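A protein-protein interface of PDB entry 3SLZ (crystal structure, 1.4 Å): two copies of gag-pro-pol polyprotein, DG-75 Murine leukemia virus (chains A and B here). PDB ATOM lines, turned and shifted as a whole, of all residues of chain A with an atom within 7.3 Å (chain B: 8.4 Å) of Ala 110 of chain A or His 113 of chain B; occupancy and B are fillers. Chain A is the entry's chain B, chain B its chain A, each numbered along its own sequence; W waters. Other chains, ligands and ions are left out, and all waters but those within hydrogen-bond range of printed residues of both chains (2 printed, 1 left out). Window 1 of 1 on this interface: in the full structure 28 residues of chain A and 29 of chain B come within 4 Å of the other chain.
The backbone carbonyl oxygen (O) of Ile 112 of chain A is in hydrogen-bond range of the backbone NH (N) of Ile 112 of chain B, at 2.8 Å.
The side-chain amide nitrogen (NE2) of Gln 111 of chain A is in hydrogen-bond range of a ring nitrogen (ND1) of His 113 of chain B (3.4 Å).
The backbone NH (N) of Phe 114 of chain B sits at hydrogen-bond distance from the backbone carbonyl oxygen (O) of Ala 110 of chain A.
The backbone NH (N) of Gln 111 of chain B sits at hydrogen-bond distance from the backbone carbonyl oxygen (O) of Val 122 of chain B, at 2.9 Å.
The side-chain amide nitrogen (NE2) of Gln 111 of chain B sits at hydrogen-bond distance from the backbone carbonyl oxygen (O) of Gly 123 of chain B (3.3 Å).
The side-chain amide oxygen of Gln 111 of chain A sits at hydrogen-bond distance from a ring nitrogen (NE2) of His 113 of chain A (2.7 Å).
Phe 114 of chain B touches Thr 106 of chain A.
Thr 106 of chain A touches Gly 116 of chain B.
Phe 114 of chain B touches Lys 109 of chain A (O to CA, 3.7 Å).
CE of Lys 109 of chain A touches O of Gly 116 of chain B (3.98 Å).
Ala 110 of chain A touches His 113 of chain B (O to C, 3.8 Å).
Gln 111 of chain A touches Ile 112 of chain B (CA to O, 3.1 Å).
Ile 112 of chain A touches Gln 111 of chain B.
Ala 110 of chain B touches His 113 of chain A.
His 113 of chain A touches Gln 111 of chain B (CE1 to OE1, 3.2 Å).
OE1 of Glu 115 of chain A touches CG of Gln 111 of chain B, 3.3 Å away.
Of chain B, only Ile 112 (3.9 Å), His 113 (3.8 Å) and Phe 114 (2.8 Å) come within 4 Å of Ala 110 of chain A.
His 113 of chain B touches just these residues of chain A: Ala 110 and Gln 111.
Gln 111 of chain A touches just these residues of chain B: Ile 112 (3.1 Å) and His 113 (3.3 Å).
Of the printed residues of chain B, Thr 106 of chain A touches Phe 114 and Gly 116.
Printed residues of chain A within 4 Å of Ile 112 of chain B: Ala 110 (3.9 Å), Gln 111 (3.1 Å) and Ile 112 (2.8 Å).
Of the printed residues of chain B, Glu 115 of chain A touches Ala 110 (3.8 Å) and Gln 111 (3.3 Å).
Of the printed residues of chain B, His 113 of chain A touches Ala 110 (3.8 Å) and Gln 111 (3.2 Å).
The nearest residue of chain B that does not touch Ala 110 of chain A is Glu 115 of chain B (5.6 Å).
The nearest printed residue of chain B that does not touch Lys 109 of chain A is Glu 115 of chain B (4.1 Å).
Of the 21 printed residues of chain B, 6 touch a printed residue of chain A.
Hydrophobic or aromatic side chains of chain A that line the printed part of chain B: Leu 105 and His 113.
Among the printed residues, no Asp or Glu carboxylate lies within 4 Å of a Lys or Arg side-chain nitrogen of the other chain.
Ala 110 of chain A touches His 113 of chain B, and with the chains exchanged His 113 of chain A touches Ala 110 of chain B.
Gln 111 of chain A touches His 113 of chain B, and with the chains exchanged His 113 of chain A touches Gln 111 of chain B.
Glu 115 of chain A touches Gln 111 of chain B, but with the chains exchanged Gln 111 of chain A does not touch Glu 115 of chain B (5.2 Å).
10 positions are printed for both chains.
Of the 17 pairs that touch across the chains among the printed residues, 9 have their exchanged pair printed and touching as well.
Water W2 lies within hydrogen-bond range of the backbone carbonyl oxygen of Gly 118 of chain B, the backbone carbonyl oxygen of Gly 116 of chain B and the side-chain hydroxyl of Thr 106 of chain A.
Water W1 lies within hydrogen-bond range of O of Ser 117 of chain B (3.1 Å) and OG1 of Thr 106 of chain A (3.2 Å).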
ATOM      1  N   ILE A  25      -9.190  18.566  -5.304  1.00  0.00           N
ATOM      2  CA  ILE A  25     -10.396  18.257  -6.087  1.00  0.00           C
ATOM      3  C   ILE A  25     -11.099  17.044  -5.489  1.00  0.00           C
ATOM      4  O   ILE A  25     -10.446  16.167  -4.962  1.00  0.00           O
ATOM      5  CB  ILE A  25     -10.074  17.956  -7.575  1.00  0.00           C
ATOM      6  CG1 ILE A  25     -11.344  17.923  -8.434  1.00  0.00           C
ATOM      7  CG2 ILE A  25      -9.219  16.719  -7.692  1.00  0.00           C
ATOM      8  CD1 ILE A  25     -11.045  17.678  -9.907  1.00  0.00           C
ATOM      9  N   VAL A  38      -4.228  17.524  -5.513  1.00  0.00           N
ATOM     10  CA  VAL A  38      -3.855  17.432  -6.908  1.00  0.00           C
ATOM     11  C   VAL A  38      -2.345  17.519  -6.955  1.00  0.00           C
ATOM     12  O   VAL A  38      -1.751  18.511  -6.498  1.00  0.00           O
ATOM     13  CB  VAL A  38      -4.510  18.563  -7.697  1.00  0.00           C
ATOM     14  CG1 VAL A  38      -3.831  18.766  -9.057  1.00  0.00           C
ATOM     15  CG2 VAL A  38      -6.019  18.253  -7.811  1.00  0.00           C
ATOM     16  N   LEU A 100      -4.083  12.873  -6.259  1.00  0.00           N
ATOM     17  CA  LEU A 100      -4.535  12.696  -7.637  1.00  0.00           C
ATOM     18  C   LEU A 100      -3.358  13.043  -8.522  1.00  0.00           C
ATOM     19  O   LEU A 100      -2.914  14.198  -8.585  1.00  0.00           O
ATOM     20  CB  LEU A 100      -5.800  13.499  -7.930  1.00  0.00           C
ATOM     21  CG  LEU A 100      -6.374  13.187  -9.311  1.00  0.00           C
ATOM     22  CD1 LEU A 100      -7.873  13.213  -9.293  1.00  0.00           C
ATOM     23  CD2 LEU A 100      -5.808  14.191 -10.288  1.00  0.00           C
ATOM     24  N   LEU A 104      -4.272  10.537 -13.608  1.00  0.00           N
ATOM     25  CA  LEU A 104      -5.640  10.994 -13.752  1.00  0.00           C
ATOM     26  C   LEU A 104      -5.691  12.436 -14.226  1.00  0.00           C
ATOM     27  O   LEU A 104      -6.699  12.860 -14.849  1.00  0.00           O
ATOM     28  CB  LEU A 104      -6.471  10.777 -12.457  1.00  0.00           C
ATOM     29  CG  LEU A 104      -6.838   9.319 -12.212  1.00  0.00           C
ATOM     30  CD1 LEU A 104      -7.530   9.156 -10.854  1.00  0.00           C
ATOM     31  CD2 LEU A 104      -7.710   8.800 -13.312  1.00  0.00           C
ATOM     32  N   LEU A 105      -4.657  13.220 -13.984  1.00  0.00           N
ATOM     33  CA  LEU A 105      -4.629  14.589 -14.534  1.00  0.00           C
ATOM     34  C   LEU A 105      -4.591  14.542 -16.048  1.00  0.00           C
ATOM     35  O   LEU A 105      -5.237  15.389 -16.700  1.00  0.00           O
ATOM     36  CB  LEU A 105      -3.442  15.352 -13.974  1.00  0.00           C
ATOM     37  CG  LEU A 105      -3.545  15.694 -12.483  1.00  0.00           C
ATOM     38  CD1 LEU A 105      -2.222  16.127 -11.872  1.00  0.00           C
ATOM     39  CD2 LEU A 105      -4.614  16.816 -12.266  1.00  0.00           C
ATOM     40  N   THR A 106      -3.916  13.541 -16.614  1.00  0.00           N
ATOM     41  CA  THR A 106      -3.922  13.361 -18.073  1.00  0.00           C
ATOM     42  C   THR A 106      -5.319  13.002 -18.551  1.00  0.00           C
ATOM     43  O   THR A 106      -5.777  13.563 -19.576  1.00  0.00           O
ATOM     44  CB  THR A 106      -2.987  12.276 -18.454  1.00  0.00           C
ATOM     45  OG1 THR A 106      -1.653  12.728 -18.238  1.00  0.00           O
ATOM     46  CG2 THR A 106      -3.137  11.941 -19.976  1.00  0.00           C
ATOM     47  N   LYS A 107      -6.022  12.130 -17.841  1.00  0.00           N
ATOM     48  CA  LYS A 107      -7.388  11.765 -18.298  1.00  0.00           C
ATOM     49  C   LYS A 107      -8.362  12.919 -18.180  1.00  0.00           C
ATOM     50  O   LYS A 107      -9.288  13.045 -18.991  1.00  0.00           O
ATOM     51  CB  LYS A 107      -7.887  10.548 -17.530  1.00  0.00           C
ATOM     52  CG  LYS A 107      -7.003   9.322 -17.760  1.00  0.00           C
ATOM     53  CD  LYS A 107      -7.605   8.069 -17.140  1.00  0.00           C
ATOM     54  CE  LYS A 107      -6.688   6.881 -17.291  1.00  0.00           C
ATOM     55  NZ  LYS A 107      -6.672   6.305 -18.661  1.00  0.00           N
ATOM     56  N   LEU A 108      -8.191  13.762 -17.169  1.00  0.00           N
ATOM     57  CA  LEU A 108      -9.034  14.940 -16.980  1.00  0.00           C
ATOM     58  C   LEU A 108      -8.669  16.094 -17.909  1.00  0.00           C
ATOM     59  O   LEU A 108      -9.436  17.059 -18.018  1.00  0.00           O
ATOM     60  CB  LEU A 108      -8.917  15.437 -15.526  1.00  0.00           C
ATOM     61  CG  LEU A 108      -9.642  14.605 -14.492  1.00  0.00           C
ATOM     62  CD1 LEU A 108      -9.085  14.850 -13.092  1.00  0.00           C
ATOM     63  CD2 LEU A 108     -11.175  14.800 -14.518  1.00  0.00           C
ATOM     64  N   LYS A 109      -7.487  16.019 -18.499  1.00  0.00           N
ATOM     65  CA  LYS A 109      -6.881  17.150 -19.225  1.00  0.00           C
ATOM     66  C   LYS A 109      -6.976  18.414 -18.378  1.00  0.00           C
ATOM     67  O   LYS A 109      -7.383  19.501 -18.833  1.00  0.00           O
ATOM     68  CB  LYS A 109      -7.556  17.344 -20.610  1.00  0.00           C
ATOM     69  CG  LYS A 109      -7.491  16.119 -21.535  1.00  0.00           C
ATOM     70  CD  LYS A 109      -6.065  15.839 -22.021  1.00  0.00           C
ATOM     71  CE  LYS A 109      -5.986  14.601 -22.926  1.00  0.00           C
ATOM     72  NZ  LYS A 109      -6.293  13.301 -22.252  1.00  0.00           N
ATOM     73  N   ALA A 110      -6.595  18.289 -17.113  1.00  0.00           N
ATOM     74  CA  ALA A 110      -6.743  19.348 -16.145  1.00  0.00           C
ATOM     75  C   ALA A 110      -5.721  20.450 -16.382  1.00  0.00           C
ATOM     76  O   ALA A 110      -4.646  20.214 -16.969  1.00  0.00           O
ATOM     77  CB  ALA A 110      -6.589  18.764 -14.720  1.00  0.00           C
ATOM     78  N   GLN A 111      -6.119  21.632 -15.934  1.00  0.00           N
ATOM     79  CA  GLN A 111      -5.191  22.766 -15.777  1.00  0.00           C
ATOM     80  C   GLN A 111      -5.160  23.121 -14.308  1.00  0.00           C
ATOM     81  O   GLN A 111      -6.175  23.143 -13.620  1.00  0.00           O
ATOM     82  CB  GLN A 111      -5.685  24.025 -16.527  1.00  0.00           C
ATOM     83  CG  GLN A 111      -5.987  23.829 -18.019  1.00  0.00           C
ATOM     84  CD  GLN A 111      -6.479  25.120 -18.661  1.00  0.00           C
ATOM     85  OE1 GLN A 111      -6.618  26.136 -18.006  1.00  0.00           O
ATOM     86  NE2 GLN A 111      -6.750  25.064 -19.956  1.00  0.00           N
ATOM     87  N   ILE A 112      -3.961  23.423 -13.810  1.00  0.00           N
ATOM     88  CA  ILE A 112      -3.807  23.874 -12.459  1.00  0.00           C
ATOM     89  C   ILE A 112      -3.269  25.311 -12.497  1.00  0.00           C
ATOM     90  O   ILE A 112      -2.248  25.565 -13.151  1.00  0.00           O
ATOM     91  CB  ILE A 112      -2.821  22.958 -11.678  1.00  0.00           C
ATOM     92  CG1 ILE A 112      -3.279  21.500 -11.736  1.00  0.00           C
ATOM     93  CG2 ILE A 112      -2.621  23.459 -10.301  1.00  0.00           C
ATOM     94  CD1 ILE A 112      -2.118  20.571 -11.684  1.00  0.00           C
ATOM     95  N   HIS A 113      -3.959  26.196 -11.793  1.00  0.00           N
ATOM     96  CA  HIS A 113      -3.651  27.640 -11.827  1.00  0.00           C
ATOM     97  C   HIS A 113      -3.272  28.155 -10.464  1.00  0.00           C
ATOM     98  O   HIS A 113      -4.049  28.027  -9.527  1.00  0.00           O
ATOM     99  CB  HIS A 113      -4.900  28.405 -12.313  1.00  0.00           C
ATOM    100  CG  HIS A 113      -5.254  28.142 -13.739  1.00  0.00           C
ATOM    101  ND1 HIS A 113      -5.194  29.125 -14.702  1.00  0.00           N
ATOM    102  CD2 HIS A 113      -5.641  27.010 -14.380  1.00  0.00           C
ATOM    103  CE1 HIS A 113      -5.549  28.616 -15.870  1.00  0.00           C
ATOM    104  NE2 HIS A 113      -5.841  27.339 -15.705  1.00  0.00           N
ATOM    105  N   GLU A 115      -2.059  31.513 -10.410  1.00  0.00           N
ATOM    106  CA  GLU A 115      -2.124  32.970 -10.691  1.00  0.00           C
ATOM    107  C   GLU A 115      -3.408  33.644 -10.190  1.00  0.00           C
ATOM    108  O   GLU A 115      -3.500  34.887 -10.170  1.00  0.00           O
ATOM    109  CB  GLU A 115      -1.957  33.215 -12.197  1.00  0.00           C
ATOM    110  CG  GLU A 115      -3.248  33.128 -13.004  1.00  0.00           C
ATOM    111  CD  GLU A 115      -3.679  31.704 -13.318  1.00  0.00           C
ATOM    112  OE1 GLU A 115      -2.967  30.732 -12.931  1.00  0.00           O
ATOM    113  OE2 GLU A 115      -4.747  31.573 -13.949  1.00  0.00           O
ATOM    114  N   VAL A 121      -8.076  24.157  -9.762  1.00  0.00           N
ATOM    115  CA  VAL A 121      -7.956  23.099 -10.750  1.00  0.00           C
ATOM    116  C   VAL A 121      -9.207  23.196 -11.613  1.00  0.00           C
ATOM    117  O   VAL A 121     -10.322  23.246 -11.092  1.00  0.00           O
ATOM    118  CB  VAL A 121      -7.911  21.681 -10.093  1.00  0.00           C
ATOM    119  CG1 VAL A 121      -7.634  20.634 -11.171  1.00  0.00           C
ATOM    120  CG2 VAL A 121      -6.867  21.682  -8.988  1.00  0.00           C
ATOM    121  N   VAL A 122      -8.962  23.265 -12.908  1.00  0.00           N
ATOM    122  CA  VAL A 122     -10.043  23.386 -13.901  1.00  0.00           C
ATOM    123  C   VAL A 122      -9.838  22.394 -15.021  1.00  0.00           C
ATOM    124  O   VAL A 122      -8.793  21.735 -15.126  1.00  0.00           O
ATOM    125  CB  VAL A 122     -10.190  24.822 -14.428  1.00  0.00           C
ATOM    126  CG1 VAL A 122     -10.641  25.757 -13.287  1.00  0.00           C
ATOM    127  CG2 VAL A 122      -8.904  25.295 -15.126  1.00  0.00           C
ATOM    128  N   GLY A 123     -10.839  22.291 -15.911  1.00  0.00           N
ATOM    129  CA  GLY A 123     -10.723  21.419 -17.061  1.00  0.00           C
ATOM    130  C   GLY A 123      -9.980  22.003 -18.252  1.00  0.00           C
ATOM    131  O   GLY A 123      -9.424  23.110 -18.169  1.00  0.00           O
ATOM    132  N   PRO A 124      -9.965  21.257 -19.371  1.00  0.00           N
ATOM    133  CA  PRO A 124      -9.160  21.613 -20.539  1.00  0.00           C
ATOM    134  C   PRO A 124      -9.506  22.946 -21.176  1.00  0.00           C
ATOM    135  O   PRO A 124      -8.659  23.527 -21.851  1.00  0.00           O
ATOM    136  CB  PRO A 124      -9.426  20.469 -21.514  1.00  0.00           C
ATOM    137  CG  PRO A 124     -10.684  19.874 -21.075  1.00  0.00           C
ATOM    138  CD  PRO A 124     -10.650  19.976 -19.573  1.00  0.00           C
ATOM    139  N   GLY A 126     -10.774  25.538 -19.157  1.00  0.00           N
ATOM    140  CA  GLY A 126     -10.789  26.553 -18.114  1.00  0.00           C
ATOM    141  C   GLY A 126     -12.003  26.407 -17.224  1.00  0.00           C
ATOM    142  O   GLY A 126     -12.184  27.181 -16.282  1.00  0.00           O
ATOM    143  N   LEU A 129     -14.303  21.687 -13.363  1.00  0.00           N
ATOM    144  CA  LEU A 129     -14.626  20.346 -13.801  1.00  0.00           C
ATOM    145  C   LEU A 129     -16.011  19.932 -13.299  1.00  0.00           C
ATOM    146  O   LEU A 129     -16.218  19.742 -12.098  1.00  0.00           O
ATOM    147  CB  LEU A 129     -13.526  19.366 -13.352  1.00  0.00           C
ATOM    148  CG  LEU A 129     -12.200  19.515 -14.121  1.00  0.00           C
ATOM    149  CD1 LEU A 129     -10.983  19.206 -13.273  1.00  0.00           C
ATOM    150  CD2 LEU A 129     -12.196  18.657 -15.377  1.00  0.00           C
ATOM    151  N   GLU B  22       7.586  15.351 -17.265  1.00  0.00           N
ATOM    152  CA  GLU B  22       6.708  16.508 -17.338  1.00  0.00           C
ATOM    153  C   GLU B  22       5.657  16.389 -16.225  1.00  0.00           C
ATOM    154  O   GLU B  22       5.234  15.290 -15.874  1.00  0.00           O
ATOM    155  CB  GLU B  22       6.011  16.589 -18.702  1.00  0.00           C
ATOM    156  CG  GLU B  22       7.017  16.693 -19.872  1.00  0.00           C
ATOM    157  CD  GLU B  22       6.334  16.918 -21.210  1.00  0.00           C
ATOM    158  OE1 GLU B  22       5.124  16.686 -21.326  1.00  0.00           O
ATOM    159  OE2 GLU B  22       7.022  17.349 -22.158  1.00  0.00           O
ATOM    160  N   PRO B  23       5.184  17.506 -15.688  1.00  0.00           N
ATOM    161  CA  PRO B  23       5.645  18.867 -16.017  1.00  0.00           C
ATOM    162  C   PRO B  23       6.973  19.215 -15.385  1.00  0.00           C
ATOM    163  O   PRO B  23       7.193  18.928 -14.202  1.00  0.00           O
ATOM    164  CB  PRO B  23       4.538  19.744 -15.462  1.00  0.00           C
ATOM    165  CG  PRO B  23       3.988  18.968 -14.240  1.00  0.00           C
ATOM    166  CD  PRO B  23       4.165  17.487 -14.630  1.00  0.00           C
ATOM    167  N   VAL B  38       7.942  19.965 -11.666  1.00  0.00           N
ATOM    168  CA  VAL B  38       6.963  20.900 -11.094  1.00  0.00           C
ATOM    169  C   VAL B  38       5.997  20.026 -10.271  1.00  0.00           C
ATOM    170  O   VAL B  38       5.352  19.080 -10.786  1.00  0.00           O
ATOM    171  CB  VAL B  38       6.221  21.588 -12.218  1.00  0.00           C
ATOM    172  CG1 VAL B  38       4.993  22.316 -11.702  1.00  0.00           C
ATOM    173  CG2 VAL B  38       7.141  22.533 -12.963  1.00  0.00           C
ATOM    174  N   ALA B 110       2.264  30.235 -11.721  1.00  0.00           N
ATOM    175  CA  ALA B 110       2.252  29.324 -12.848  1.00  0.00           C
ATOM    176  C   ALA B 110       0.896  28.684 -13.135  1.00  0.00           C
ATOM    177  O   ALA B 110       0.074  28.526 -12.228  1.00  0.00           O
ATOM    178  CB  ALA B 110       3.247  28.218 -12.629  1.00  0.00           C
ATOM    179  N   GLN B 111       0.706  28.307 -14.386  1.00  0.00           N
ATOM    180  CA  GLN B 111      -0.389  27.391 -14.735  1.00  0.00           C
ATOM    181  C   GLN B 111       0.280  26.174 -15.306  1.00  0.00           C
ATOM    182  O   GLN B 111       1.296  26.250 -15.967  1.00  0.00           O
ATOM    183  CB  GLN B 111      -1.321  27.989 -15.802  1.00  0.00           C
ATOM    184  CG  GLN B 111      -1.587  29.462 -15.641  1.00  0.00           C
ATOM    185  CD  GLN B 111      -2.390  30.054 -16.757  1.00  0.00           C
ATOM    186  OE1 GLN B 111      -2.900  29.353 -17.595  1.00  0.00           O
ATOM    187  NE2 GLN B 111      -2.516  31.357 -16.751  1.00  0.00           N
ATOM    188  N   ILE B 112      -0.328  25.025 -15.053  1.00  0.00           N
ATOM    189  CA  ILE B 112       0.175  23.743 -15.512  1.00  0.00           C
ATOM    190  C   ILE B 112      -0.950  23.123 -16.308  1.00  0.00           C
ATOM    191  O   ILE B 112      -2.064  22.947 -15.782  1.00  0.00           O
ATOM    192  CB  ILE B 112       0.568  22.833 -14.335  1.00  0.00           C
ATOM    193  CG1 ILE B 112       1.574  23.557 -13.425  1.00  0.00           C
ATOM    194  CG2 ILE B 112       1.122  21.546 -14.853  1.00  0.00           C
ATOM    195  CD1 ILE B 112       1.483  23.231 -12.004  1.00  0.00           C
ATOM    196  N   HIS B 113      -0.649  22.778 -17.541  1.00  0.00           N
ATOM    197  CA  HIS B 113      -1.678  22.293 -18.474  1.00  0.00           C
ATOM    198  C   HIS B 113      -1.412  20.879 -18.900  1.00  0.00           C
ATOM    199  O   HIS B 113      -0.380  20.599 -19.493  1.00  0.00           O
ATOM    200  CB  HIS B 113      -1.700  23.216 -19.722  1.00  0.00           C
ATOM    201  CG  HIS B 113      -2.223  24.586 -19.453  1.00  0.00           C
ATOM    202  ND1 HIS B 113      -3.350  25.072 -20.076  1.00  0.00           N
ATOM    203  CD2 HIS B 113      -1.776  25.583 -18.655  1.00  0.00           C
ATOM    204  CE1 HIS B 113      -3.575  26.311 -19.673  1.00  0.00           C
ATOM    205  NE2 HIS B 113      -2.638  26.649 -18.805  1.00  0.00           N
ATOM    206  N   PHE B 114      -2.356  19.983 -18.641  1.00  0.00           N
ATOM    207  CA  PHE B 114      -2.202  18.596 -19.078  1.00  0.00           C
ATOM    208  C   PHE B 114      -2.794  18.472 -20.476  1.00  0.00           C
ATOM    209  O   PHE B 114      -3.933  18.848 -20.694  1.00  0.00           O
ATOM    210  CB  PHE B 114      -2.791  17.611 -18.027  1.00  0.00           C
ATOM    211  CG  PHE B 114      -1.866  17.393 -16.857  1.00  0.00           C
ATOM    212  CD1 PHE B 114      -1.058  16.272 -16.828  1.00  0.00           C
ATOM    213  CD2 PHE B 114      -1.732  18.350 -15.867  1.00  0.00           C
ATOM    214  CE1 PHE B 114      -0.143  16.071 -15.769  1.00  0.00           C
ATOM    215  CE2 PHE B 114      -0.830  18.180 -14.810  1.00  0.00           C
ATOM    216  CZ  PHE B 114      -0.033  17.058 -14.768  1.00  0.00           C
ATOM    217  N   GLU B 115      -1.953  18.087 -21.435  1.00  0.00           N
ATOM    218  CA  GLU B 115      -2.376  17.972 -22.853  1.00  0.00           C
ATOM    219  C   GLU B 115      -1.565  16.905 -23.571  1.00  0.00           C
ATOM    220  O   GLU B 115      -0.346  16.812 -23.390  1.00  0.00           O
ATOM    221  CB  GLU B 115      -2.249  19.308 -23.615  1.00  0.00           C
ATOM    222  CG  GLU B 115      -3.207  20.443 -23.198  1.00  0.00           C
ATOM    223  CD  GLU B 115      -4.694  20.087 -23.310  1.00  0.00           C
ATOM    224  OE1 GLU B 115      -5.505  20.706 -22.579  1.00  0.00           O
ATOM    225  OE2 GLU B 115      -5.057  19.196 -24.119  1.00  0.00           O
ATOM    226  N   GLY B 116      -2.235  16.111 -24.399  1.00  0.00           N
ATOM    227  CA  GLY B 116      -1.616  14.906 -24.935  1.00  0.00           C
ATOM    228  C   GLY B 116      -1.270  13.980 -23.782  1.00  0.00           C
ATOM    229  O   GLY B 116      -2.086  13.793 -22.864  1.00  0.00           O
ATOM    230  N   SER B 117      -0.058  13.426 -23.819  1.00  0.00           N
ATOM    231  CA  SER B 117       0.418  12.499 -22.784  1.00  0.00           C
ATOM    232  C   SER B 117       1.280  13.196 -21.728  1.00  0.00           C
ATOM    233  O   SER B 117       1.692  12.585 -20.737  1.00  0.00           O
ATOM    234  CB  SER B 117       1.199  11.334 -23.412  1.00  0.00           C
ATOM    235  OG  SER B 117       2.375  11.786 -24.075  1.00  0.00           O
ATOM    236  N   GLY B 118       1.538  14.480 -21.947  1.00  0.00           N
ATOM    237  CA  GLY B 118       2.402  15.241 -21.067  1.00  0.00           C
ATOM    238  C   GLY B 118       1.731  16.462 -20.484  1.00  0.00           C
ATOM    239  O   GLY B 118       0.508  16.494 -20.266  1.00  0.00           O
ATOM    240  N   ALA B 119       2.539  17.479 -20.240  1.00  0.00           N
ATOM    241  CA  ALA B 119       2.083  18.579 -19.419  1.00  0.00           C
ATOM    242  C   ALA B 119       3.013  19.720 -19.661  1.00  0.00           C
ATOM    243  O   ALA B 119       4.200  19.527 -19.772  1.00  0.00           O
ATOM    244  CB  ALA B 119       2.114  18.170 -17.955  1.00  0.00           C
ATOM    245  N   GLN B 120       2.450  20.917 -19.721  1.00  0.00           N
ATOM    246  CA  GLN B 120       3.287  22.085 -19.931  1.00  0.00           C
ATOM    247  C   GLN B 120       3.035  23.161 -18.910  1.00  0.00           C
ATOM    248  O   GLN B 120       1.957  23.274 -18.341  1.00  0.00           O
ATOM    249  CB  GLN B 120       3.224  22.661 -21.355  1.00  0.00           C
ATOM    250  CG  GLN B 120       1.871  22.636 -22.016  1.00  0.00           C
ATOM    251  CD  GLN B 120       1.629  21.350 -22.799  1.00  0.00           C
ATOM    252  OE1 GLN B 120       0.483  20.999 -23.091  1.00  0.00           O
ATOM    253  NE2 GLN B 120       2.706  20.640 -23.132  1.00  0.00           N
ATOM    254  N   VAL B 121       4.059  23.981 -18.736  1.00  0.00           N
ATOM    255  CA  VAL B 121       4.048  25.056 -17.758  1.00  0.00           C
ATOM    256  C   VAL B 121       3.947  26.403 -18.502  1.00  0.00           C
ATOM    257  O   VAL B 121       4.716  26.639 -19.457  1.00  0.00           O
ATOM    258  CB  VAL B 121       5.292  24.959 -16.899  1.00  0.00           C
ATOM    259  CG1 VAL B 121       5.295  26.045 -15.826  1.00  0.00           C
ATOM    260  CG2 VAL B 121       5.409  23.535 -16.272  1.00  0.00           C
ATOM    261  N   VAL B 122       3.009  27.238 -18.048  1.00  0.00           N
ATOM    262  CA  VAL B 122       2.766  28.579 -18.600  1.00  0.00           C
ATOM    263  C   VAL B 122       2.746  29.635 -17.468  1.00  0.00           C
ATOM    264  O   VAL B 122       2.567  29.314 -16.299  1.00  0.00           O
ATOM    265  CB  VAL B 122       1.481  28.651 -19.499  1.00  0.00           C
ATOM    266  CG1 VAL B 122       1.377  27.468 -20.469  1.00  0.00           C
ATOM    267  CG2 VAL B 122       0.239  28.771 -18.679  1.00  0.00           C
ATOM    268  N   GLY B 123       2.973  30.905 -17.795  1.00  0.00           N
ATOM    269  CA  GLY B 123       3.078  31.944 -16.777  1.00  0.00           C
ATOM    270  C   GLY B 123       1.730  32.561 -16.456  1.00  0.00           C
ATOM    271  O   GLY B 123       0.696  32.151 -17.015  1.00  0.00           O
ATOM    272  N   GLY B 126      -0.537  33.603 -19.264  1.00  0.00           N
ATOM    273  CA  GLY B 126      -0.725  32.601 -20.306  1.00  0.00           C
ATOM    274  C   GLY B 126       0.421  32.426 -21.286  1.00  0.00           C
ATOM    275  O   GLY B 126       0.270  31.700 -22.258  1.00  0.00           O
ATOM    276  N   GLN B 127       1.547  33.095 -21.062  1.00  0.00           N
ATOM    277  CA  GLN B 127       2.716  32.925 -21.922  1.00  0.00           C
ATOM    278  C   GLN B 127       3.320  31.539 -21.672  1.00  0.00           C
ATOM    279  O   GLN B 127       3.509  31.168 -20.530  1.00  0.00           O
ATOM    280  CB  GLN B 127       3.753  34.038 -21.655  1.00  0.00           C
ATOM    281  CG  GLN B 127       4.620  33.875 -20.366  1.00  0.00           C
ATOM    282  CD  GLN B 127       4.071  34.562 -19.110  1.00  0.00           C
ATOM    283  OE1 GLN B 127       4.846  35.074 -18.299  1.00  0.00           O
ATOM    284  NE2 GLN B 127       2.745  34.570 -18.937  1.00  0.00           N
ATOM    285  N   PRO B 128       3.596  30.745 -22.727  1.00  0.00           N
ATOM    286  CA  PRO B 128       4.283  29.487 -22.396  1.00  0.00           C
ATOM    287  C   PRO B 128       5.642  29.787 -21.778  1.00  0.00           C
ATOM    288  O   PRO B 128       6.295  30.762 -22.173  1.00  0.00           O
ATOM    289  CB  PRO B 128       4.448  28.801 -23.762  1.00  0.00           C
ATOM    290  CG  PRO B 128       3.368  29.420 -24.630  1.00  0.00           C
ATOM    291  CD  PRO B 128       3.319  30.859 -24.172  1.00  0.00           C
ATOM    292  N   GLN B 130       7.978  27.453 -21.820  1.00  0.00           N
ATOM    293  CA  GLN B 130       8.821  26.414 -22.407  1.00  0.00           C
ATOM    294  C   GLN B 130       8.270  25.969 -23.747  1.00  0.00           C
ATOM    295  O   GLN B 130       7.218  26.460 -24.198  1.00  0.00           O
ATOM    296  CB  GLN B 130       8.929  25.224 -21.445  1.00  0.00           C
ATOM    297  CG  GLN B 130       7.554  24.695 -21.052  1.00  0.00           C
ATOM    298  CD  GLN B 130       7.574  23.657 -19.965  1.00  0.00           C
ATOM    299  OE1 GLN B 130       6.550  23.028 -19.718  1.00  0.00           O
ATOM    300  NE2 GLN B 130       8.727  23.459 -19.315  1.00  0.00           N
HETATM  301  O   HOH W   1       1.516  13.133 -17.646  1.00  0.00           O
HETATM  302  O   HOH W   2      -1.400  14.818 -20.313  1.00  0.00           O
